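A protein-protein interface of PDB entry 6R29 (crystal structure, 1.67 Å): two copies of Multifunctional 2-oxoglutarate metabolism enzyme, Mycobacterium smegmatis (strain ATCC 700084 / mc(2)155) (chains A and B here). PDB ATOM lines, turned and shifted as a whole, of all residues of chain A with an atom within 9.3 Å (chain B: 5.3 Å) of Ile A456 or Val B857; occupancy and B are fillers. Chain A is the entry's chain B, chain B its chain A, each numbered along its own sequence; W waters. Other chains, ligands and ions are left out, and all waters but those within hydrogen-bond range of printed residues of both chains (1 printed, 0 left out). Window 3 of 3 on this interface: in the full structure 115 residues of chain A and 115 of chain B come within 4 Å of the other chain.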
ATOM      1  N   GLU A 203     -11.887   4.666  19.901  1.00  0.00           N
ATOM      2  CA  GLU A 203     -12.119   4.223  18.523  1.00  0.00           C
ATOM      3  C   GLU A 203     -11.353   5.080  17.522  1.00  0.00           C
ATOM      4  O   GLU A 203     -11.089   4.624  16.409  1.00  0.00           O
ATOM      5  CB  GLU A 203     -13.627   4.273  18.190  1.00  0.00           C
ATOM      6  CG  GLU A 203     -14.440   3.151  18.821  1.00  0.00           C
ATOM      7  CD  GLU A 203     -14.086   1.748  18.362  1.00  0.00           C
ATOM      8  OE1 GLU A 203     -13.979   1.527  17.135  1.00  0.00           O
ATOM      9  OE2 GLU A 203     -13.911   0.869  19.233  1.00  0.00           O
ATOM     10  N   GLY A 204     -11.060   6.320  17.898  1.00  0.00           N
ATOM     11  CA  GLY A 204     -10.412   7.290  17.021  1.00  0.00           C
ATOM     12  C   GLY A 204     -11.370   7.723  15.929  1.00  0.00           C
ATOM     13  O   GLY A 204     -10.965   7.936  14.786  1.00  0.00           O
ATOM     14  N   ASN A 205     -12.668   7.792  16.268  1.00  0.00           N
ATOM     15  CA  ASN A 205     -13.720   8.200  15.342  1.00  0.00           C
ATOM     16  C   ASN A 205     -14.394   9.412  15.940  1.00  0.00           C
ATOM     17  O   ASN A 205     -15.395   9.300  16.652  1.00  0.00           O
ATOM     18  CB  ASN A 205     -14.702   7.059  15.061  1.00  0.00           C
ATOM     19  CG  ASN A 205     -15.636   7.381  13.919  1.00  0.00           C
ATOM     20  OD1 ASN A 205     -15.328   8.221  13.052  1.00  0.00           O
ATOM     21  ND2 ASN A 205     -16.797   6.728  13.902  1.00  0.00           N
ATOM     22  N   LEU A 206     -13.776  10.573  15.708  1.00  0.00           N
ATOM     23  CA  LEU A 206     -14.194  11.852  16.267  1.00  0.00           C
ATOM     24  C   LEU A 206     -14.996  12.682  15.273  1.00  0.00           C
ATOM     25  O   LEU A 206     -14.587  12.821  14.116  1.00  0.00           O
ATOM     26  CB  LEU A 206     -12.941  12.643  16.718  1.00  0.00           C
ATOM     27  CG  LEU A 206     -11.886  11.892  17.569  1.00  0.00           C
ATOM     28  CD1 LEU A 206     -10.634  12.732  17.737  1.00  0.00           C
ATOM     29  CD2 LEU A 206     -12.443  11.475  18.939  1.00  0.00           C
ATOM     30  N   ALA A 211     -12.814  16.843  16.856  1.00  0.00           N
ATOM     31  CA  ALA A 211     -11.553  16.916  16.106  1.00  0.00           C
ATOM     32  C   ALA A 211     -11.075  18.369  15.872  1.00  0.00           C
ATOM     33  O   ALA A 211     -10.063  18.582  15.190  1.00  0.00           O
ATOM     34  CB  ALA A 211     -11.700  16.194  14.774  1.00  0.00           C
ATOM     35  N   LYS A 453     -17.640   6.168   9.914  1.00  0.00           N
ATOM     36  CA  LYS A 453     -16.257   6.605  10.136  1.00  0.00           C
ATOM     37  C   LYS A 453     -15.943   7.879   9.354  1.00  0.00           C
ATOM     38  O   LYS A 453     -16.231   7.962   8.160  1.00  0.00           O
ATOM     39  CB  LYS A 453     -15.242   5.501   9.768  1.00  0.00           C
ATOM     40  CG  LYS A 453     -15.610   4.091  10.233  1.00  0.00           C
ATOM     41  CD  LYS A 453     -15.146   3.775  11.646  1.00  0.00           C
ATOM     42  CE  LYS A 453     -15.643   2.419  12.085  1.00  0.00           C
ATOM     43  NZ  LYS A 453     -17.008   2.491  12.676  1.00  0.00           N
ATOM     44  N   HIS A 454     -15.365   8.872  10.042  1.00  0.00           N
ATOM     45  CA  HIS A 454     -14.954  10.152   9.458  1.00  0.00           C
ATOM     46  C   HIS A 454     -13.554  10.018   8.858  1.00  0.00           C
ATOM     47  O   HIS A 454     -12.720   9.313   9.435  1.00  0.00           O
ATOM     48  CB  HIS A 454     -14.955  11.260  10.536  1.00  0.00           C
ATOM     49  CG  HIS A 454     -16.282  11.471  11.204  1.00  0.00           C
ATOM     50  ND1 HIS A 454     -17.286  12.212  10.602  1.00  0.00           N
ATOM     51  CD2 HIS A 454     -16.725  11.031  12.406  1.00  0.00           C
ATOM     52  CE1 HIS A 454     -18.304  12.193  11.449  1.00  0.00           C
ATOM     53  NE2 HIS A 454     -18.017  11.489  12.545  1.00  0.00           N
ATOM     54  N   GLU A 455     -13.285  10.687   7.714  1.00  0.00           N
ATOM     55  CA  GLU A 455     -11.941  10.697   7.110  1.00  0.00           C
ATOM     56  C   GLU A 455     -11.002  11.477   8.022  1.00  0.00           C
ATOM     57  O   GLU A 455     -11.425  12.481   8.604  1.00  0.00           O
ATOM     58  CB  GLU A 455     -11.956  11.313   5.707  1.00  0.00           C
ATOM     59  N   ILE A 456      -9.764  11.007   8.184  1.00  0.00           N
ATOM     60  CA  ILE A 456      -8.802  11.671   9.068  1.00  0.00           C
ATOM     61  C   ILE A 456      -8.048  12.718   8.265  1.00  0.00           C
ATOM     62  O   ILE A 456      -7.483  12.412   7.218  1.00  0.00           O
ATOM     63  CB  ILE A 456      -7.840  10.674   9.772  1.00  0.00           C
ATOM     64  CG1 ILE A 456      -8.618   9.575  10.509  1.00  0.00           C
ATOM     65  CG2 ILE A 456      -6.889  11.391  10.743  1.00  0.00           C
ATOM     66  CD1 ILE A 456      -8.247   8.296  10.085  1.00  0.00           C
ATOM     67  N   GLU A 457      -8.031  13.948   8.770  1.00  0.00           N
ATOM     68  CA  GLU A 457      -7.360  15.062   8.116  1.00  0.00           C
ATOM     69  C   GLU A 457      -6.289  15.668   9.019  1.00  0.00           C
ATOM     70  O   GLU A 457      -6.415  15.588  10.249  1.00  0.00           O
ATOM     71  CB  GLU A 457      -8.399  16.153   7.750  1.00  0.00           C
ATOM     72  CG  GLU A 457      -9.358  15.747   6.641  1.00  0.00           C
ATOM     73  CD  GLU A 457     -10.536  16.669   6.372  1.00  0.00           C
ATOM     74  OE1 GLU A 457     -10.776  17.600   7.174  1.00  0.00           O
ATOM     75  OE2 GLU A 457     -11.234  16.441   5.357  1.00  0.00           O
ATOM     76  N   PRO A 458      -5.263  16.357   8.457  1.00  0.00           N
ATOM     77  CA  PRO A 458      -4.308  17.073   9.330  1.00  0.00           C
ATOM     78  C   PRO A 458      -5.047  18.106  10.192  1.00  0.00           C
ATOM     79  O   PRO A 458      -6.089  18.618   9.769  1.00  0.00           O
ATOM     80  CB  PRO A 458      -3.374  17.769   8.333  1.00  0.00           C
ATOM     81  CG  PRO A 458      -3.510  16.992   7.070  1.00  0.00           C
ATOM     82  CD  PRO A 458      -4.951  16.577   7.029  1.00  0.00           C
ATOM     83  N   SER A 459      -4.546  18.387  11.396  1.00  0.00           N
ATOM     84  CA  SER A 459      -5.183  19.368  12.274  1.00  0.00           C
ATOM     85  C   SER A 459      -5.125  20.769  11.643  1.00  0.00           C
ATOM     86  O   SER A 459      -4.239  21.044  10.817  1.00  0.00           O
ATOM     87  CB  SER A 459      -4.528  19.368  13.653  1.00  0.00           C
ATOM     88  OG  SER A 459      -3.226  19.928  13.592  1.00  0.00           O
ATOM     89  N   LYS B 853      -3.973   9.121  14.974  1.00  0.00           N
ATOM     90  CA  LYS B 853      -4.378   8.998  13.573  1.00  0.00           C
ATOM     91  C   LYS B 853      -4.058  10.279  12.783  1.00  0.00           C
ATOM     92  O   LYS B 853      -3.632  10.205  11.622  1.00  0.00           O
ATOM     93  CB  LYS B 853      -5.868   8.656  13.470  1.00  0.00           C
ATOM     94  CG  LYS B 853      -6.182   7.251  13.980  1.00  0.00           C
ATOM     95  CD  LYS B 853      -7.657   6.897  13.796  1.00  0.00           C
ATOM     96  CE  LYS B 853      -7.969   5.495  14.264  1.00  0.00           C
ATOM     97  NZ  LYS B 853      -9.394   5.145  14.014  1.00  0.00           N
ATOM     98  N   VAL B 854      -4.239  11.448  13.418  1.00  0.00           N
ATOM     99  CA  VAL B 854      -3.940  12.746  12.787  1.00  0.00           C
ATOM    100  C   VAL B 854      -2.420  12.857  12.596  1.00  0.00           C
ATOM    101  O   VAL B 854      -1.973  13.246  11.520  1.00  0.00           O
ATOM    102  CB  VAL B 854      -4.525  13.938  13.593  1.00  0.00           C
ATOM    103  CG1 VAL B 854      -4.031  15.273  13.038  1.00  0.00           C
ATOM    104  CG2 VAL B 854      -6.056  13.897  13.585  1.00  0.00           C
ATOM    105  N   HIS B 855      -1.631  12.450  13.616  1.00  0.00           N
ATOM    106  CA  HIS B 855      -0.179  12.426  13.503  1.00  0.00           C
ATOM    107  C   HIS B 855       0.238  11.635  12.250  1.00  0.00           C
ATOM    108  O   HIS B 855       1.088  12.091  11.491  1.00  0.00           O
ATOM    109  CB  HIS B 855       0.456  11.779  14.757  1.00  0.00           C
ATOM    110  CG  HIS B 855       1.785  11.132  14.481  1.00  0.00           C
ATOM    111  ND1 HIS B 855       2.937  11.888  14.336  1.00  0.00           N
ATOM    112  CD2 HIS B 855       2.085   9.828  14.254  1.00  0.00           C
ATOM    113  CE1 HIS B 855       3.903  11.027  14.046  1.00  0.00           C
ATOM    114  NE2 HIS B 855       3.435   9.774  13.969  1.00  0.00           N
ATOM    115  N   ALA B 856      -0.337  10.424  12.071  1.00  0.00           N
ATOM    116  CA  ALA B 856       0.035   9.528  10.984  1.00  0.00           C
ATOM    117  C   ALA B 856      -0.210  10.144   9.588  1.00  0.00           C
ATOM    118  O   ALA B 856       0.648  10.000   8.720  1.00  0.00           O
ATOM    119  CB  ALA B 856      -0.697   8.211  11.117  1.00  0.00           C
ATOM    120  N   VAL B 857      -1.341  10.852   9.401  1.00  0.00           N
ATOM    121  CA  VAL B 857      -1.687  11.503   8.129  1.00  0.00           C
ATOM    122  C   VAL B 857      -0.709  12.648   7.860  1.00  0.00           C
ATOM    123  O   VAL B 857      -0.228  12.793   6.725  1.00  0.00           O
ATOM    124  CB  VAL B 857      -3.163  11.985   8.106  1.00  0.00           C
ATOM    125  CG1 VAL B 857      -3.450  12.866   6.888  1.00  0.00           C
ATOM    126  CG2 VAL B 857      -4.118  10.799   8.145  1.00  0.00           C
ATOM    127  N   GLU B 858      -0.404  13.453   8.905  1.00  0.00           N
ATOM    128  CA  GLU B 858       0.541  14.557   8.780  1.00  0.00           C
ATOM    129  C   GLU B 858       1.939  14.045   8.445  1.00  0.00           C
ATOM    130  O   GLU B 858       2.632  14.661   7.639  1.00  0.00           O
ATOM    131  CB  GLU B 858       0.595  15.372  10.076  1.00  0.00           C
ATOM    132  CG  GLU B 858      -0.679  16.122  10.401  1.00  0.00           C
ATOM    133  CD  GLU B 858      -0.664  16.728  11.799  1.00  0.00           C
ATOM    134  OE1 GLU B 858       0.273  16.420  12.576  1.00  0.00           O
ATOM    135  OE2 GLU B 858      -1.608  17.484  12.130  1.00  0.00           O
ATOM    136  N   GLN B 859       2.353  12.918   9.053  1.00  0.00           N
ATOM    137  CA  GLN B 859       3.679  12.332   8.813  1.00  0.00           C
ATOM    138  C   GLN B 859       3.815  11.884   7.357  1.00  0.00           C
ATOM    139  O   GLN B 859       4.858  12.106   6.733  1.00  0.00           O
ATOM    140  CB  GLN B 859       3.916  11.135   9.748  1.00  0.00           C
ATOM    141  CG  GLN B 859       5.373  10.659   9.800  1.00  0.00           C
ATOM    142  CD  GLN B 859       6.239  11.477  10.748  1.00  0.00           C
ATOM    143  OE1 GLN B 859       5.813  12.481  11.325  1.00  0.00           O
ATOM    144  NE2 GLN B 859       7.481  11.058  10.933  1.00  0.00           N
ATOM    145  N   GLN B 860       2.761  11.250   6.819  1.00  0.00           N
ATOM    146  CA  GLN B 860       2.758  10.770   5.440  1.00  0.00           C
ATOM    147  C   GLN B 860       2.813  11.951   4.459  1.00  0.00           C
ATOM    148  O   GLN B 860       3.461  11.830   3.415  1.00  0.00           O
ATOM    149  CB  GLN B 860       1.534   9.878   5.180  1.00  0.00           C
ATOM    150  CG  GLN B 860       1.622   9.031   3.895  1.00  0.00           C
ATOM    151  CD  GLN B 860       2.914   8.248   3.772  1.00  0.00           C
ATOM    152  OE1 GLN B 860       3.729   8.537   2.899  1.00  0.00           O
ATOM    153  NE2 GLN B 860       3.152   7.264   4.637  1.00  0.00           N
ATOM    154  N   GLU B 861       2.178  13.099   4.803  1.00  0.00           N
ATOM    155  CA  GLU B 861       2.220  14.316   3.970  1.00  0.00           C
ATOM    156  C   GLU B 861       3.648  14.814   3.793  1.00  0.00           C
ATOM    157  O   GLU B 861       4.002  15.253   2.702  1.00  0.00           O
ATOM    158  CB  GLU B 861       1.403  15.454   4.583  1.00  0.00           C
ATOM    159  CG  GLU B 861      -0.088  15.414   4.325  1.00  0.00           C
ATOM    160  CD  GLU B 861      -0.792  16.700   4.715  1.00  0.00           C
ATOM    161  OE1 GLU B 861      -1.687  17.132   3.955  1.00  0.00           O
ATOM    162  OE2 GLU B 861      -0.451  17.280   5.774  1.00  0.00           O
HETATM  163  O   HOH W   1     -12.658   4.125  14.150  1.00  0.00           O
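O of Lys B853 touches CG2 of Ile A456, at 3.6 Å.
N of Val B854 touches CG2 of Ile A456 (3.8 Å).
CG2 of Ile A456 touches CG2 of Val B857, 3.8 Å away.
Glu A457 touches Val B854.
Pro A458 touches Glu B858.
Glu B861 touches Pro A458 (OE2 to CG, 3.3 Å).
Ser A459 touches Val B854.
Of the 9 printed residues of chain B, 5 touch a printed residue of chain A.
Printed residues of chain B that touch a printed residue of chain A: Lys B853, Val B854, Val B857, Glu B858 and Glu B861.
Hydrophobic or aromatic side chains of chain B that line the printed part of chain A: Val B854 and Val B857.
Hydrophobic or aromatic side chains of chain A within 4 Å of the printed part of chain B: Ile A456 and Pro A458.
Among the printed residues, no Asp or Glu carboxylate lies within 4 Å of a Lys or Arg side-chain nitrogen of the other chain.
Asn A205 touches none of the printed residues of chain B.
Leu A206 touches none of the printed residues of chain B.
Ile A456 touches just these residues of chain B: Lys B853, Val B854 and Val B857.
Of the printed residues of chain A, Lys B853 touches Glu A203 (3.0 Å), Gly A204 (3.3 Å) and Ile A456 (3.6 Å).
Of the printed residues of chain A, Val B854 touches Ile A456 (3.8 Å), Glu A457 (3.7 Å) and Ser A459 (3.6 Å).
Printed residues of chain A within 4 Å of Val B857: Ile A456.
The nearest printed residue of chain A that does not touch Val B857 is Pro A458 (4.01 Å).
N of Ser A459 lies within hydrogen-bond range of OE2 of Glu B858 (3.2 Å).
The backbone carbonyl oxygen of Gly A204 is in hydrogen-bond range of the side-chain amino group of Lys B853, 3.3 Å away.
The backbone carbonyl oxygen of Glu A203 lies within hydrogen-bond range of the side-chain amino group of Lys B853 (3.0 Å).
No position is printed for both chains.
Water W1 lies within hydrogen-bond range of the backbone carbonyl oxygen (O) of Glu A203 (2.8 Å) and the side-chain amino group (NZ) of Lys B853 (3.4 Å).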
